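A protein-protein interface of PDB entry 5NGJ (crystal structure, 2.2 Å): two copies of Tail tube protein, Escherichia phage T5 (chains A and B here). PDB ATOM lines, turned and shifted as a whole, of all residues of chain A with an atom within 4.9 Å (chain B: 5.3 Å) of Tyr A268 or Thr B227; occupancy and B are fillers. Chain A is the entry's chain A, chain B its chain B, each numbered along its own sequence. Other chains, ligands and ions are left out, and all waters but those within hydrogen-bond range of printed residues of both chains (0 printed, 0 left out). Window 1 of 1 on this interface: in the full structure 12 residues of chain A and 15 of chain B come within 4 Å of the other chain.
ND2 of Asn A270 sits at hydrogen-bond distance from OH of Tyr B268 (3.3 Å).
The side-chain hydroxyl (OG) of Ser A273 sits at hydrogen-bond distance from the backbone carbonyl oxygen (O) of Tyr A268.
OH of Tyr A268 is in hydrogen-bond range of O of Val A329, at 2.7 Å.
N of Ser A273 lies within hydrogen-bond range of OD1 of Asn A270 (3.1 Å).
N of Ile B161 sits at hydrogen-bond distance from O of Thr B227, 3.3 Å away.
The backbone carbonyl oxygen (O) of Pro B225 sits at hydrogen-bond distance from the backbone NH (N) of Tyr B268 (3.0 Å).
The backbone carbonyl oxygen (O) of Thr B266 sits at hydrogen-bond distance from the backbone NH (N) of Thr B227.
Among the printed residues, pairs that only touch across the chains: Tyr A268 with Tyr B268, Ser A273 with Val B329, Asn A270 with Val B329, Tyr A268 with Thr B227, Leu A330 with Ile B161, Val A329 with Thr B227, Pro A225 with Leu B330 and Tyr A268 with Val B329.
Of the printed residues of chain B, Pro A225 touches Leu B330.
Thr A227 touches none of the printed residues of chain B.
Printed residues of chain B within 4 Å of Tyr A268: Thr B227 (3.5 Å), Tyr B268 (3.3 Å) and Val B329 (3.98 Å).
Printed residues of chain B within 4 Å of Ser A273: Val B329.
Of the printed residues of chain B, Leu A330 touches Ile B161 (3.7 Å).
Printed residues of chain A within 4 Å of Ile B161: Leu A330 (3.7 Å).
Thr B227 touches two residues of chain A.
Printed residues of chain A within 4 Å of Tyr B268: Tyr A268 (3.3 Å) and Asn A270 (3.3 Å).
The nearest printed residue of chain A that does not touch Thr B227 is Leu A330 (5.9 Å).
Of the 13 printed residues of chain B, 5 touch a printed residue of chain A.
Hydrophobic or aromatic side chains of chain A within 4 Å of the printed part of chain B: Pro A225, Tyr A268 and Leu A330.
Among the printed residues, no Asp or Glu carboxylate lies within 4 Å of a Lys or Arg side-chain nitrogen of the other chain.
Pro A225 touches Leu B330, but with the chains exchanged Leu A330 does not touch Pro B225 (8.5 Å).
Tyr A268 touches Thr B227, but with the chains exchanged Thr A227 does not touch Tyr B268 (7.8 Å).
Tyr A268 touches its own counterpart, Tyr B268.
Val A329 touches Thr B227, but with the chains exchanged Thr A227 does not touch Val B329 (6.2 Å).
Of the 9 pairs that touch across the chains among the printed residues, 1 has its exchanged pair printed and touching as well.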
ATOM      1  N   PRO A 225     -19.721  -4.637 -34.303  1.00  0.00           N
ATOM      2  CA  PRO A 225     -20.511  -3.927 -33.282  1.00  0.00           C
ATOM      3  C   PRO A 225     -19.650  -3.444 -32.128  1.00  0.00           C
ATOM      4  O   PRO A 225     -18.817  -4.194 -31.632  1.00  0.00           O
ATOM      5  CB  PRO A 225     -21.527  -4.985 -32.817  1.00  0.00           C
ATOM      6  CG  PRO A 225     -21.503  -6.036 -33.863  1.00  0.00           C
ATOM      7  CD  PRO A 225     -20.105  -6.061 -34.362  1.00  0.00           C
ATOM      8  N   THR A 227     -19.617  -1.710 -28.293  1.00  0.00           N
ATOM      9  CA  THR A 227     -20.359  -1.551 -27.044  1.00  0.00           C
ATOM     10  C   THR A 227     -19.757  -0.501 -26.119  1.00  0.00           C
ATOM     11  O   THR A 227     -20.444  -0.034 -25.218  1.00  0.00           O
ATOM     12  CB  THR A 227     -20.395  -2.887 -26.323  1.00  0.00           C
ATOM     13  OG1 THR A 227     -19.048  -3.308 -26.116  1.00  0.00           O
ATOM     14  CG2 THR A 227     -21.158  -3.942 -27.113  1.00  0.00           C
ATOM     15  N   THR A 266     -14.272  -1.070 -27.526  1.00  0.00           N
ATOM     16  CA  THR A 266     -14.558  -2.439 -27.098  1.00  0.00           C
ATOM     17  C   THR A 266     -15.639  -2.991 -27.998  1.00  0.00           C
ATOM     18  O   THR A 266     -16.706  -2.392 -28.125  1.00  0.00           O
ATOM     19  CB  THR A 266     -14.980  -2.507 -25.643  1.00  0.00           C
ATOM     20  OG1 THR A 266     -13.947  -1.923 -24.855  1.00  0.00           O
ATOM     21  CG2 THR A 266     -15.230  -3.949 -25.187  1.00  0.00           C
ATOM     22  N   ALA A 267     -15.381  -4.152 -28.594  1.00  0.00           N
ATOM     23  CA  ALA A 267     -16.313  -4.800 -29.493  1.00  0.00           C
ATOM     24  C   ALA A 267     -16.695  -6.169 -29.031  1.00  0.00           C
ATOM     25  O   ALA A 267     -15.978  -6.802 -28.264  1.00  0.00           O
ATOM     26  CB  ALA A 267     -15.673  -4.927 -30.850  1.00  0.00           C
ATOM     27  N   TYR A 268     -17.823  -6.643 -29.531  1.00  0.00           N
ATOM     28  CA  TYR A 268     -18.237  -8.015 -29.315  1.00  0.00           C
ATOM     29  C   TYR A 268     -18.064  -8.625 -30.686  1.00  0.00           C
ATOM     30  O   TYR A 268     -18.801  -8.321 -31.625  1.00  0.00           O
ATOM     31  CB  TYR A 268     -19.626  -8.143 -28.687  1.00  0.00           C
ATOM     32  CG  TYR A 268     -19.516  -8.081 -27.173  1.00  0.00           C
ATOM     33  CD1 TYR A 268     -19.438  -9.243 -26.418  1.00  0.00           C
ATOM     34  CD2 TYR A 268     -19.260  -6.876 -26.525  1.00  0.00           C
ATOM     35  CE1 TYR A 268     -19.250  -9.198 -25.036  1.00  0.00           C
ATOM     36  CE2 TYR A 268     -19.065  -6.820 -25.149  1.00  0.00           C
ATOM     37  CZ  TYR A 268     -19.068  -7.981 -24.407  1.00  0.00           C
ATOM     38  OH  TYR A 268     -18.870  -7.877 -23.054  1.00  0.00           O
ATOM     39  N   LEU A 269     -16.935  -9.321 -30.809  1.00  0.00           N
ATOM     40  CA  LEU A 269     -16.398  -9.928 -32.019  1.00  0.00           C
ATOM     41  C   LEU A 269     -16.378 -11.444 -31.936  1.00  0.00           C
ATOM     42  O   LEU A 269     -15.583 -12.006 -31.182  1.00  0.00           O
ATOM     43  CB  LEU A 269     -14.957  -9.434 -32.234  1.00  0.00           C
ATOM     44  CG  LEU A 269     -14.758  -8.430 -33.309  1.00  0.00           C
ATOM     45  CD1 LEU A 269     -13.398  -7.792 -33.167  1.00  0.00           C
ATOM     46  CD2 LEU A 269     -14.885  -9.056 -34.669  1.00  0.00           C
ATOM     47  N   ASN A 270     -17.129 -12.086 -32.845  1.00  0.00           N
ATOM     48  CA  ASN A 270     -17.240 -13.536 -32.975  1.00  0.00           C
ATOM     49  C   ASN A 270     -18.136 -13.883 -34.188  1.00  0.00           C
ATOM     50  O   ASN A 270     -18.555 -12.986 -34.922  1.00  0.00           O
ATOM     51  CB  ASN A 270     -17.749 -14.172 -31.663  1.00  0.00           C
ATOM     52  CG  ASN A 270     -18.973 -13.526 -31.071  1.00  0.00           C
ATOM     53  OD1 ASN A 270     -20.005 -13.402 -31.734  1.00  0.00           O
ATOM     54  ND2 ASN A 270     -18.911 -13.149 -29.791  1.00  0.00           N
ATOM     55  N   SER A 273     -21.930 -12.254 -33.895  1.00  0.00           N
ATOM     56  CA  SER A 273     -21.920 -10.793 -34.021  1.00  0.00           C
ATOM     57  C   SER A 273     -21.638 -10.261 -35.429  1.00  0.00           C
ATOM     58  O   SER A 273     -22.266  -9.290 -35.839  1.00  0.00           O
ATOM     59  CB  SER A 273     -20.943 -10.173 -33.022  1.00  0.00           C
ATOM     60  OG  SER A 273     -19.597 -10.286 -33.449  1.00  0.00           O
ATOM     61  N   ASP A 328     -14.061 -13.472 -25.091  1.00  0.00           N
ATOM     62  CA  ASP A 328     -14.332 -13.387 -23.653  1.00  0.00           C
ATOM     63  C   ASP A 328     -15.386 -12.335 -23.274  1.00  0.00           C
ATOM     64  O   ASP A 328     -15.788 -11.501 -24.095  1.00  0.00           O
ATOM     65  CB  ASP A 328     -13.014 -13.132 -22.896  1.00  0.00           C
ATOM     66  CG  ASP A 328     -12.331 -11.814 -23.233  1.00  0.00           C
ATOM     67  OD1 ASP A 328     -11.943 -11.090 -22.288  1.00  0.00           O
ATOM     68  OD2 ASP A 328     -12.155 -11.522 -24.444  1.00  0.00           O
ATOM     69  N   VAL A 329     -15.832 -12.406 -22.004  1.00  0.00           N
ATOM     70  CA  VAL A 329     -16.832 -11.506 -21.402  1.00  0.00           C
ATOM     71  C   VAL A 329     -16.418 -10.048 -21.407  1.00  0.00           C
ATOM     72  O   VAL A 329     -17.300  -9.204 -21.319  1.00  0.00           O
ATOM     73  CB  VAL A 329     -17.267 -11.911 -19.966  1.00  0.00           C
ATOM     74  CG1 VAL A 329     -18.007 -13.244 -19.964  1.00  0.00           C
ATOM     75  CG2 VAL A 329     -16.086 -11.921 -18.996  1.00  0.00           C
ATOM     76  N   LEU A 330     -15.102  -9.737 -21.447  1.00  0.00           N
ATOM     77  CA  LEU A 330     -14.650  -8.342 -21.489  1.00  0.00           C
ATOM     78  C   LEU A 330     -14.731  -7.748 -22.919  1.00  0.00           C
ATOM     79  O   LEU A 330     -14.339  -6.591 -23.117  1.00  0.00           O
ATOM     80  CB  LEU A 330     -13.216  -8.185 -20.932  1.00  0.00           C
ATOM     81  CG  LEU A 330     -12.927  -8.777 -19.552  1.00  0.00           C
ATOM     82  CD1 LEU A 330     -11.507  -8.439 -19.114  1.00  0.00           C
ATOM     83  CD2 LEU A 330     -13.906  -8.267 -18.509  1.00  0.00           C
ATOM     84  N   GLY A 331     -15.232  -8.531 -23.886  1.00  0.00           N
ATOM     85  CA  GLY A 331     -15.306  -8.102 -25.275  1.00  0.00           C
ATOM     86  C   GLY A 331     -13.918  -8.111 -25.868  1.00  0.00           C
ATOM     87  O   GLY A 331     -13.045  -8.819 -25.373  1.00  0.00           O
ATOM     88  N   VAL B 159     -22.068  -1.718 -11.824  1.00  0.00           N
ATOM     89  CA  VAL B 159     -21.763  -3.105 -12.136  1.00  0.00           C
ATOM     90  C   VAL B 159     -21.146  -3.197 -13.556  1.00  0.00           C
ATOM     91  O   VAL B 159     -21.179  -4.239 -14.203  1.00  0.00           O
ATOM     92  CB  VAL B 159     -23.066  -3.937 -11.952  1.00  0.00           C
ATOM     93  CG1 VAL B 159     -22.856  -5.378 -12.276  1.00  0.00           C
ATOM     94  CG2 VAL B 159     -23.573  -3.816 -10.533  1.00  0.00           C
ATOM     95  N   ASP B 160     -20.570  -2.120 -14.023  1.00  0.00           N
ATOM     96  CA  ASP B 160     -19.847  -2.093 -15.282  1.00  0.00           C
ATOM     97  C   ASP B 160     -18.534  -2.815 -15.015  1.00  0.00           C
ATOM     98  O   ASP B 160     -17.851  -2.461 -14.049  1.00  0.00           O
ATOM     99  CB  ASP B 160     -19.571  -0.651 -15.730  1.00  0.00           C
ATOM    100  CG  ASP B 160     -18.786  -0.552 -17.016  1.00  0.00           C
ATOM    101  OD1 ASP B 160     -19.295  -1.018 -18.060  1.00  0.00           O
ATOM    102  OD2 ASP B 160     -17.668   0.006 -16.987  1.00  0.00           O
ATOM    103  N   ILE B 161     -18.215  -3.852 -15.826  1.00  0.00           N
ATOM    104  CA  ILE B 161     -16.990  -4.674 -15.698  1.00  0.00           C
ATOM    105  C   ILE B 161     -15.703  -3.873 -15.574  1.00  0.00           C
ATOM    106  O   ILE B 161     -14.754  -4.380 -14.984  1.00  0.00           O
ATOM    107  CB  ILE B 161     -16.810  -5.723 -16.844  1.00  0.00           C
ATOM    108  CG1 ILE B 161     -17.172  -5.143 -18.224  1.00  0.00           C
ATOM    109  CG2 ILE B 161     -17.559  -6.991 -16.534  1.00  0.00           C
ATOM    110  CD1 ILE B 161     -16.293  -5.621 -19.341  1.00  0.00           C
ATOM    111  N   PRO B 225     -23.669 -14.068 -16.509  1.00  0.00           N
ATOM    112  CA  PRO B 225     -22.621 -13.036 -16.483  1.00  0.00           C
ATOM    113  C   PRO B 225     -23.167 -11.649 -16.793  1.00  0.00           C
ATOM    114  O   PRO B 225     -23.942 -11.493 -17.728  1.00  0.00           O
ATOM    115  CB  PRO B 225     -21.632 -13.502 -17.557  1.00  0.00           C
ATOM    116  CG  PRO B 225     -21.972 -14.919 -17.815  1.00  0.00           C
ATOM    117  CD  PRO B 225     -23.433 -15.015 -17.616  1.00  0.00           C
ATOM    118  N   ILE B 226     -22.779 -10.660 -15.978  1.00  0.00           N
ATOM    119  CA  ILE B 226     -23.210  -9.269 -16.122  1.00  0.00           C
ATOM    120  C   ILE B 226     -22.002  -8.419 -16.564  1.00  0.00           C
ATOM    121  O   ILE B 226     -20.925  -8.483 -15.963  1.00  0.00           O
ATOM    122  CB  ILE B 226     -23.846  -8.764 -14.806  1.00  0.00           C
ATOM    123  CG1 ILE B 226     -25.029  -9.650 -14.367  1.00  0.00           C
ATOM    124  CG2 ILE B 226     -24.275  -7.281 -14.896  1.00  0.00           C
ATOM    125  CD1 ILE B 226     -26.184  -9.817 -15.378  1.00  0.00           C
ATOM    126  N   THR B 227     -22.201  -7.656 -17.628  1.00  0.00           N
ATOM    127  CA  THR B 227     -21.192  -6.775 -18.192  1.00  0.00           C
ATOM    128  C   THR B 227     -21.461  -5.301 -17.902  1.00  0.00           C
ATOM    129  O   THR B 227     -20.550  -4.485 -18.052  1.00  0.00           O
ATOM    130  CB  THR B 227     -21.126  -6.990 -19.701  1.00  0.00           C
ATOM    131  OG1 THR B 227     -22.430  -6.762 -20.233  1.00  0.00           O
ATOM    132  CG2 THR B 227     -20.665  -8.383 -20.050  1.00  0.00           C
ATOM    133  N   GLY B 228     -22.670  -4.965 -17.488  1.00  0.00           N
ATOM    134  CA  GLY B 228     -22.975  -3.583 -17.217  1.00  0.00           C
ATOM    135  C   GLY B 228     -24.236  -3.372 -16.437  1.00  0.00           C
ATOM    136  O   GLY B 228     -24.959  -4.315 -16.146  1.00  0.00           O
ATOM    137  N   GLY B 229     -24.455  -2.119 -16.093  1.00  0.00           N
ATOM    138  CA  GLY B 229     -25.629  -1.667 -15.376  1.00  0.00           C
ATOM    139  C   GLY B 229     -25.346  -1.167 -13.989  1.00  0.00           C
ATOM    140  O   GLY B 229     -24.201  -0.851 -13.615  1.00  0.00           O
ATOM    141  N   THR B 266     -27.156  -5.436 -17.874  1.00  0.00           N
ATOM    142  CA  THR B 266     -26.922  -5.969 -19.213  1.00  0.00           C
ATOM    143  C   THR B 266     -26.135  -7.237 -19.022  1.00  0.00           C
ATOM    144  O   THR B 266     -25.062  -7.222 -18.401  1.00  0.00           O
ATOM    145  CB  THR B 266     -26.194  -5.002 -20.122  1.00  0.00           C
ATOM    146  OG1 THR B 266     -26.966  -3.808 -20.203  1.00  0.00           O
ATOM    147  CG2 THR B 266     -26.000  -5.577 -21.512  1.00  0.00           C
ATOM    148  N   ALA B 267     -26.735  -8.349 -19.473  1.00  0.00           N
ATOM    149  CA  ALA B 267     -26.174  -9.682 -19.344  1.00  0.00           C
ATOM    150  C   ALA B 267     -25.634 -10.201 -20.654  1.00  0.00           C
ATOM    151  O   ALA B 267     -26.171  -9.869 -21.708  1.00  0.00           O
ATOM    152  CB  ALA B 267     -27.255 -10.629 -18.840  1.00  0.00           C
ATOM    153  N   TYR B 268     -24.599 -11.052 -20.590  1.00  0.00           N
ATOM    154  CA  TYR B 268     -24.083 -11.741 -21.772  1.00  0.00           C
ATOM    155  C   TYR B 268     -24.791 -13.116 -21.701  1.00  0.00           C
ATOM    156  O   TYR B 268     -24.363 -13.958 -20.914  1.00  0.00           O
ATOM    157  CB  TYR B 268     -22.537 -11.846 -21.755  1.00  0.00           C
ATOM    158  CG  TYR B 268     -21.968 -12.167 -23.124  1.00  0.00           C
ATOM    159  CD1 TYR B 268     -22.122 -11.283 -24.190  1.00  0.00           C
ATOM    160  CD2 TYR B 268     -21.316 -13.372 -23.367  1.00  0.00           C
ATOM    161  CE1 TYR B 268     -21.632 -11.586 -25.461  1.00  0.00           C
ATOM    162  CE2 TYR B 268     -20.818 -13.686 -24.637  1.00  0.00           C
ATOM    163  CZ  TYR B 268     -20.967 -12.781 -25.680  1.00  0.00           C
ATOM    164  OH  TYR B 268     -20.488 -13.048 -26.947  1.00  0.00           O
ATOM    165  N   VAL B 329     -26.139 -11.621 -29.360  1.00  0.00           N
ATOM    166  CA  VAL B 329     -24.762 -11.344 -28.925  1.00  0.00           C
ATOM    167  C   VAL B 329     -24.409  -9.873 -28.533  1.00  0.00           C
ATOM    168  O   VAL B 329     -23.267  -9.653 -28.130  1.00  0.00           O
ATOM    169  CB  VAL B 329     -23.832 -11.830 -30.057  1.00  0.00           C
ATOM    170  CG1 VAL B 329     -23.938 -10.927 -31.287  1.00  0.00           C
ATOM    171  CG2 VAL B 329     -22.389 -12.003 -29.579  1.00  0.00           C
ATOM    172  N   LEU B 330     -25.332  -8.893 -28.589  1.00  0.00           N
ATOM    173  CA  LEU B 330     -24.974  -7.521 -28.199  1.00  0.00           C
ATOM    174  C   LEU B 330     -25.007  -7.375 -26.684  1.00  0.00           C
ATOM    175  O   LEU B 330     -24.023  -6.974 -26.055  1.00  0.00           O
ATOM    176  CB  LEU B 330     -25.917  -6.488 -28.840  1.00  0.00           C
ATOM    177  CG  LEU B 330     -25.592  -6.079 -30.276  1.00  0.00           C
ATOM    178  CD1 LEU B 330     -24.257  -5.345 -30.356  1.00  0.00           C
ATOM    179  CD2 LEU B 330     -25.627  -7.291 -31.233  1.00  0.00           C
